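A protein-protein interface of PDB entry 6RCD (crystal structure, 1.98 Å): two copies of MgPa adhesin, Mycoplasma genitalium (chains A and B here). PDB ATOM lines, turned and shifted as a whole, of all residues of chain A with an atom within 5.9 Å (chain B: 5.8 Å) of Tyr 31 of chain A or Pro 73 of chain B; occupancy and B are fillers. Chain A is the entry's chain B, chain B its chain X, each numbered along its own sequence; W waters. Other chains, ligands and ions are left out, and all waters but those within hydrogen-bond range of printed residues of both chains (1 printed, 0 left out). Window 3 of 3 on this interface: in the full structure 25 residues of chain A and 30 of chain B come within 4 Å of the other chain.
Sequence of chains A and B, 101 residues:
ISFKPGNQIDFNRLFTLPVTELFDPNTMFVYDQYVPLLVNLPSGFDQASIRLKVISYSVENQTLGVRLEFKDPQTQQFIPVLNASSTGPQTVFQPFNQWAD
Water W1 bridges the side-chain carboxylate of Glu 21 of chain A (2.7 Å) and the side-chain carboxylate of Asp 72 of chain B (3.0 Å).
The backbone carbonyl oxygen (O) of Leu 22 of chain A is in hydrogen-bond range of the backbone NH (N) of Tyr 31 of chain A (3.0 Å). N of Asp 24 of chain A lies within hydrogen-bond range of O of Phe 29 of chain A (3.0 Å). OD1 of Asp 72 of chain B sits at hydrogen-bond distance from N of Gln 74 of chain B, 3.0 Å away. The side-chain amide nitrogen (NE2) of Gln 76 of chain B is in hydrogen-bond range of the backbone carbonyl oxygen (O) of Pro 73 of chain B (2.9 Å).
Among the printed residues, merely in contact across the chains: Tyr 34 of chain A with Phe 70 of chain B, Tyr 31 of chain A with Pro 73 of chain B, Gln 33 of chain A with Pro 73 of chain B, Tyr 34 of chain A with Pro 73 of chain B and Asp 24 of chain A with Gln 74 of chain B.
No position is printed for both chains. Of the 7 pairs that touch across the chains among the printed residues, none has its exchanged pair printed and touching as well.
Of the printed residues of chain B, Asp 24 of chain A touches Gln 74. Phe 29 of chain A touches none of the printed residues of chain B. Val 30 of chain A touches none of the printed residues of chain B. Tyr 31 of chain A touches two residues of chain B. Printed residues of chain B within 4 Å of Gln 33 of chain A: Lys 71 and Pro 73. Of the printed residues of chain B, Tyr 34 of chain A touches Phe 70 and Pro 73. Of the printed residues of chain A, Phe 70 of chain B touches Tyr 34. Of the printed residues of chain A, Gln 74 of chain B touches Asp 24 and Tyr 31. The nearest residue of chain A that does not touch Pro 73 of chain B is Glu 21 of chain A (4.9 Å). The nearest printed residue of chain B that does not touch Tyr 34 of chain A is Lys 71 of chain B (4.1 Å).
Of the 7 printed residues of chain B, 4 touch a printed residue of chain A. Printed residues of chain A that touch a printed residue of chain B: Asp 24, Tyr 31, Gln 33 and Tyr 34. Hydrophobic or aromatic side chains of chain A within 4 Å of the printed part of chain B: Tyr 31 and Tyr 34. Along chain A the printed residues that touch a printed residue of chain B span positions 24 to 34. Among the printed residues, no Asp or Glu carboxylate lies within 4 Å of a Lys or Arg side-chain nitrogen of the other chain.
The side-chain amide oxygen (OE1) of Gln 74 of chain B lies within hydrogen-bond range of the side-chain hydroxyl (OH) of Tyr 31 of chain A (3.1 Å). The side-chain amide oxygen of Gln 33 of chain A lies close to the backbone carbonyl oxygen of Lys 71 of chain B, at 3.1 Å.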
ATOM      1  N   THR A  20     -13.184   1.404   3.935  1.00  0.00           N
ATOM      2  CA  THR A  20     -12.545   0.065   3.963  1.00  0.00           C
ATOM      3  C   THR A  20     -11.048   0.114   4.305  1.00  0.00           C
ATOM      4  O   THR A  20     -10.475  -0.901   4.709  1.00  0.00           O
ATOM      5  CB  THR A  20     -12.809  -0.699   2.642  1.00  0.00           C
ATOM      6  OG1 THR A  20     -12.441   0.119   1.541  1.00  0.00           O
ATOM      7  CG2 THR A  20     -14.253  -1.048   2.447  1.00  0.00           C
ATOM      8  N   GLU A  21     -10.419   1.286   4.161  1.00  0.00           N
ATOM      9  CA  GLU A  21      -9.007   1.467   4.462  1.00  0.00           C
ATOM     10  C   GLU A  21      -8.769   1.931   5.901  1.00  0.00           C
ATOM     11  O   GLU A  21      -7.621   2.044   6.315  1.00  0.00           O
ATOM     12  CB  GLU A  21      -8.380   2.453   3.444  1.00  0.00           C
ATOM     13  CG  GLU A  21      -8.422   1.960   1.995  1.00  0.00           C
ATOM     14  CD  GLU A  21      -7.803   0.594   1.739  1.00  0.00           C
ATOM     15  OE1 GLU A  21      -6.634   0.376   2.136  1.00  0.00           O
ATOM     16  OE2 GLU A  21      -8.498  -0.272   1.158  1.00  0.00           O
ATOM     17  N   LEU A  22      -9.835   2.186   6.669  1.00  0.00           N
ATOM     18  CA  LEU A  22      -9.697   2.714   8.038  1.00  0.00           C
ATOM     19  C   LEU A  22      -9.426   1.652   9.115  1.00  0.00           C
ATOM     20  O   LEU A  22      -9.047   2.004  10.232  1.00  0.00           O
ATOM     21  CB  LEU A  22     -10.969   3.504   8.411  1.00  0.00           C
ATOM     22  CG  LEU A  22     -11.199   4.852   7.674  1.00  0.00           C
ATOM     23  CD1 LEU A  22     -12.607   5.364   7.936  1.00  0.00           C
ATOM     24  CD2 LEU A  22     -10.170   5.903   8.089  1.00  0.00           C
ATOM     25  N   PHE A  23      -9.651   0.376   8.795  1.00  0.00           N
ATOM     26  CA  PHE A  23      -9.519  -0.720   9.771  1.00  0.00           C
ATOM     27  C   PHE A  23      -8.774  -1.916   9.238  1.00  0.00           C
ATOM     28  O   PHE A  23      -8.712  -2.123   8.029  1.00  0.00           O
ATOM     29  CB  PHE A  23     -10.914  -1.148  10.286  1.00  0.00           C
ATOM     30  CG  PHE A  23     -11.828  -1.658   9.194  1.00  0.00           C
ATOM     31  CD1 PHE A  23     -12.614  -0.774   8.450  1.00  0.00           C
ATOM     32  CD2 PHE A  23     -11.917  -3.019   8.920  1.00  0.00           C
ATOM     33  CE1 PHE A  23     -13.442  -1.238   7.430  1.00  0.00           C
ATOM     34  CE2 PHE A  23     -12.735  -3.481   7.883  1.00  0.00           C
ATOM     35  CZ  PHE A  23     -13.488  -2.585   7.145  1.00  0.00           C
ATOM     36  N   ASP A  24      -8.186  -2.692  10.157  1.00  0.00           N
ATOM     37  CA  ASP A  24      -7.499  -3.937   9.844  1.00  0.00           C
ATOM     38  C   ASP A  24      -8.603  -5.008   9.775  1.00  0.00           C
ATOM     39  O   ASP A  24      -9.180  -5.327  10.813  1.00  0.00           O
ATOM     40  CB  ASP A  24      -6.477  -4.300  10.957  1.00  0.00           C
ATOM     41  CG  ASP A  24      -5.691  -5.587  10.702  1.00  0.00           C
ATOM     42  OD1 ASP A  24      -6.004  -6.309   9.714  1.00  0.00           O
ATOM     43  OD2 ASP A  24      -4.754  -5.859  11.460  1.00  0.00           O
ATOM     44  N   PRO A  25      -8.947  -5.548   8.588  1.00  0.00           N
ATOM     45  CA  PRO A  25     -10.025  -6.562   8.535  1.00  0.00           C
ATOM     46  C   PRO A  25      -9.723  -7.897   9.239  1.00  0.00           C
ATOM     47  O   PRO A  25     -10.647  -8.666   9.516  1.00  0.00           O
ATOM     48  CB  PRO A  25     -10.278  -6.742   7.047  1.00  0.00           C
ATOM     49  CG  PRO A  25      -9.033  -6.313   6.382  1.00  0.00           C
ATOM     50  CD  PRO A  25      -8.392  -5.267   7.246  1.00  0.00           C
ATOM     51  N   PHE A  29     -10.540  -3.872  14.000  1.00  0.00           N
ATOM     52  CA  PHE A  29     -10.317  -2.654  14.786  1.00  0.00           C
ATOM     53  C   PHE A  29      -9.773  -1.574  13.852  1.00  0.00           C
ATOM     54  O   PHE A  29      -8.962  -1.861  12.972  1.00  0.00           O
ATOM     55  CB  PHE A  29      -9.372  -2.874  15.993  1.00  0.00           C
ATOM     56  CG  PHE A  29      -9.990  -3.668  17.116  1.00  0.00           C
ATOM     57  CD1 PHE A  29     -10.889  -3.072  18.006  1.00  0.00           C
ATOM     58  CD2 PHE A  29      -9.694  -5.012  17.278  1.00  0.00           C
ATOM     59  CE1 PHE A  29     -11.511  -3.823  19.004  1.00  0.00           C
ATOM     60  CE2 PHE A  29     -10.292  -5.757  18.304  1.00  0.00           C
ATOM     61  CZ  PHE A  29     -11.189  -5.154  19.162  1.00  0.00           C
ATOM     62  N   VAL A  30     -10.219  -0.338  14.055  1.00  0.00           N
ATOM     63  CA  VAL A  30      -9.728   0.839  13.327  1.00  0.00           C
ATOM     64  C   VAL A  30      -8.221   0.927  13.631  1.00  0.00           C
ATOM     65  O   VAL A  30      -7.822   0.694  14.783  1.00  0.00           O
ATOM     66  CB  VAL A  30     -10.491   2.117  13.798  1.00  0.00           C
ATOM     67  CG1 VAL A  30      -9.820   3.400  13.289  1.00  0.00           C
ATOM     68  CG2 VAL A  30     -11.961   2.073  13.365  1.00  0.00           C
ATOM     69  N   TYR A  31      -7.386   1.193  12.593  1.00  0.00           N
ATOM     70  CA  TYR A  31      -5.945   1.340  12.793  1.00  0.00           C
ATOM     71  C   TYR A  31      -5.697   2.482  13.790  1.00  0.00           C
ATOM     72  O   TYR A  31      -6.373   3.524  13.710  1.00  0.00           O
ATOM     73  CB  TYR A  31      -5.249   1.701  11.460  1.00  0.00           C
ATOM     74  CG  TYR A  31      -5.246   0.588  10.454  1.00  0.00           C
ATOM     75  CD1 TYR A  31      -4.461  -0.553  10.648  1.00  0.00           C
ATOM     76  CD2 TYR A  31      -5.979   0.686   9.275  1.00  0.00           C
ATOM     77  CE1 TYR A  31      -4.417  -1.570   9.700  1.00  0.00           C
ATOM     78  CE2 TYR A  31      -5.935  -0.327   8.311  1.00  0.00           C
ATOM     79  CZ  TYR A  31      -5.154  -1.452   8.536  1.00  0.00           C
ATOM     80  OH  TYR A  31      -5.105  -2.482   7.632  1.00  0.00           O
ATOM     81  N   ASP A  32      -4.746   2.290  14.728  1.00  0.00           N
ATOM     82  CA  ASP A  32      -4.403   3.283  15.755  1.00  0.00           C
ATOM     83  C   ASP A  32      -4.248   4.701  15.227  1.00  0.00           C
ATOM     84  O   ASP A  32      -4.777   5.629  15.846  1.00  0.00           O
ATOM     85  CB  ASP A  32      -3.110   2.897  16.498  1.00  0.00           C
ATOM     86  CG  ASP A  32      -3.170   1.608  17.296  1.00  0.00           C
ATOM     87  OD1 ASP A  32      -4.291   1.176  17.650  1.00  0.00           O
ATOM     88  OD2 ASP A  32      -2.091   1.049  17.597  1.00  0.00           O
ATOM     89  N   GLN A  33      -3.541   4.877  14.086  1.00  0.00           N
ATOM     90  CA  GLN A  33      -3.281   6.210  13.511  1.00  0.00           C
ATOM     91  C   GLN A  33      -4.544   6.971  13.107  1.00  0.00           C
ATOM     92  O   GLN A  33      -4.496   8.193  13.007  1.00  0.00           O
ATOM     93  CB  GLN A  33      -2.281   6.113  12.329  1.00  0.00           C
ATOM     94  CG  GLN A  33      -2.892   5.523  11.052  1.00  0.00           C
ATOM     95  CD  GLN A  33      -1.905   4.985  10.043  1.00  0.00           C
ATOM     96  OE1 GLN A  33      -1.766   5.505   8.928  1.00  0.00           O
ATOM     97  NE2 GLN A  33      -1.356   3.831  10.322  1.00  0.00           N
ATOM     98  N   TYR A  34      -5.672   6.263  12.846  1.00  0.00           N
ATOM     99  CA  TYR A  34      -6.926   6.915  12.443  1.00  0.00           C
ATOM    100  C   TYR A  34      -7.907   7.188  13.583  1.00  0.00           C
ATOM    101  O   TYR A  34      -8.859   7.939  13.381  1.00  0.00           O
ATOM    102  CB  TYR A  34      -7.638   6.162  11.318  1.00  0.00           C
ATOM    103  CG  TYR A  34      -6.785   5.922  10.092  1.00  0.00           C
ATOM    104  CD1 TYR A  34      -6.013   6.952   9.531  1.00  0.00           C
ATOM    105  CD2 TYR A  34      -6.766   4.676   9.469  1.00  0.00           C
ATOM    106  CE1 TYR A  34      -5.232   6.735   8.396  1.00  0.00           C
ATOM    107  CE2 TYR A  34      -6.007   4.451   8.323  1.00  0.00           C
ATOM    108  CZ  TYR A  34      -5.240   5.483   7.789  1.00  0.00           C
ATOM    109  OH  TYR A  34      -4.477   5.235   6.666  1.00  0.00           O
ATOM    110  N   VAL A  35      -7.695   6.605  14.762  1.00  0.00           N
ATOM    111  CA  VAL A  35      -8.580   6.849  15.915  1.00  0.00           C
ATOM    112  C   VAL A  35      -8.732   8.385  16.185  1.00  0.00           C
ATOM    113  O   VAL A  35      -9.875   8.818  16.212  1.00  0.00           O
ATOM    114  CB  VAL A  35      -8.203   6.026  17.165  1.00  0.00           C
ATOM    115  CG1 VAL A  35      -9.011   6.454  18.389  1.00  0.00           C
ATOM    116  CG2 VAL A  35      -8.373   4.520  16.906  1.00  0.00           C
ATOM    117  N   PHE B  70      -0.315   9.636   2.744  1.00  0.00           N
ATOM    118  CA  PHE B  70      -0.464   8.948   4.020  1.00  0.00           C
ATOM    119  C   PHE B  70       0.226   7.582   3.958  1.00  0.00           C
ATOM    120  O   PHE B  70       0.321   6.976   2.884  1.00  0.00           O
ATOM    121  CB  PHE B  70      -1.946   8.833   4.427  1.00  0.00           C
ATOM    122  CG  PHE B  70      -2.737   7.808   3.628  1.00  0.00           C
ATOM    123  CD1 PHE B  70      -3.215   8.107   2.352  1.00  0.00           C
ATOM    124  CD2 PHE B  70      -2.993   6.543   4.146  1.00  0.00           C
ATOM    125  CE1 PHE B  70      -3.921   7.148   1.603  1.00  0.00           C
ATOM    126  CE2 PHE B  70      -3.693   5.582   3.401  1.00  0.00           C
ATOM    127  CZ  PHE B  70      -4.141   5.887   2.128  1.00  0.00           C
ATOM    128  N   LYS B  71       0.704   7.108   5.121  1.00  0.00           N
ATOM    129  CA  LYS B  71       1.395   5.830   5.227  1.00  0.00           C
ATOM    130  C   LYS B  71       0.367   4.715   5.282  1.00  0.00           C
ATOM    131  O   LYS B  71      -0.441   4.676   6.216  1.00  0.00           O
ATOM    132  CB  LYS B  71       2.275   5.824   6.486  1.00  0.00           C
ATOM    133  CG  LYS B  71       3.316   4.700   6.512  1.00  0.00           C
ATOM    134  CD  LYS B  71       4.234   4.768   7.743  1.00  0.00           C
ATOM    135  CE  LYS B  71       3.602   4.710   9.124  1.00  0.00           C
ATOM    136  NZ  LYS B  71       4.493   5.289  10.174  1.00  0.00           N
ATOM    137  N   ASP B  72       0.361   3.846   4.273  1.00  0.00           N
ATOM    138  CA  ASP B  72      -0.547   2.693   4.238  1.00  0.00           C
ATOM    139  C   ASP B  72      -0.173   1.786   5.430  1.00  0.00           C
ATOM    140  O   ASP B  72       0.980   1.370   5.517  1.00  0.00           O
ATOM    141  CB  ASP B  72      -0.406   1.947   2.910  1.00  0.00           C
ATOM    142  CG  ASP B  72      -1.333   0.759   2.784  1.00  0.00           C
ATOM    143  OD1 ASP B  72      -1.056  -0.278   3.419  1.00  0.00           O
ATOM    144  OD2 ASP B  72      -2.324   0.864   2.040  1.00  0.00           O
ATOM    145  N   PRO B  73      -1.089   1.523   6.395  1.00  0.00           N
ATOM    146  CA  PRO B  73      -0.693   0.734   7.582  1.00  0.00           C
ATOM    147  C   PRO B  73      -0.260  -0.699   7.314  1.00  0.00           C
ATOM    148  O   PRO B  73       0.504  -1.233   8.115  1.00  0.00           O
ATOM    149  CB  PRO B  73      -1.912   0.798   8.498  1.00  0.00           C
ATOM    150  CG  PRO B  73      -3.020   1.221   7.626  1.00  0.00           C
ATOM    151  CD  PRO B  73      -2.481   1.995   6.491  1.00  0.00           C
ATOM    152  N   GLN B  74      -0.688  -1.296   6.189  1.00  0.00           N
ATOM    153  CA  GLN B  74      -0.321  -2.663   5.844  1.00  0.00           C
ATOM    154  C   GLN B  74       1.033  -2.743   5.136  1.00  0.00           C
ATOM    155  O   GLN B  74       1.847  -3.594   5.496  1.00  0.00           O
ATOM    156  CB  GLN B  74      -1.413  -3.350   5.002  1.00  0.00           C
ATOM    157  CG  GLN B  74      -2.679  -3.747   5.776  1.00  0.00           C
ATOM    158  CD  GLN B  74      -2.495  -4.816   6.841  1.00  0.00           C
ATOM    159  OE1 GLN B  74      -2.928  -4.658   7.991  1.00  0.00           O
ATOM    160  NE2 GLN B  74      -1.861  -5.929   6.486  1.00  0.00           N
ATOM    161  N   THR B  75       1.269  -1.887   4.117  1.00  0.00           N
ATOM    162  CA  THR B  75       2.510  -1.913   3.332  1.00  0.00           C
ATOM    163  C   THR B  75       3.626  -1.024   3.893  1.00  0.00           C
ATOM    164  O   THR B  75       4.778  -1.184   3.494  1.00  0.00           O
ATOM    165  CB  THR B  75       2.242  -1.575   1.861  1.00  0.00           C
ATOM    166  OG1 THR B  75       1.885  -0.191   1.748  1.00  0.00           O
ATOM    167  CG2 THR B  75       1.175  -2.472   1.227  1.00  0.00           C
ATOM    168  N   GLN B  76       3.280  -0.060   4.769  1.00  0.00           N
ATOM    169  CA  GLN B  76       4.203   0.916   5.376  1.00  0.00           C
ATOM    170  C   GLN B  76       4.813   1.879   4.330  1.00  0.00           C
ATOM    171  O   GLN B  76       5.839   2.529   4.574  1.00  0.00           O
ATOM    172  CB  GLN B  76       5.278   0.232   6.252  1.00  0.00           C
ATOM    173  CG  GLN B  76       4.719  -0.430   7.509  1.00  0.00           C
ATOM    174  CD  GLN B  76       4.119   0.573   8.453  1.00  0.00           C
ATOM    175  OE1 GLN B  76       4.763   1.547   8.857  1.00  0.00           O
ATOM    176  NE2 GLN B  76       2.855   0.368   8.802  1.00  0.00           N
HETATM  177  O   HOH W   1      -4.828   2.327   2.731  1.00  0.00           O
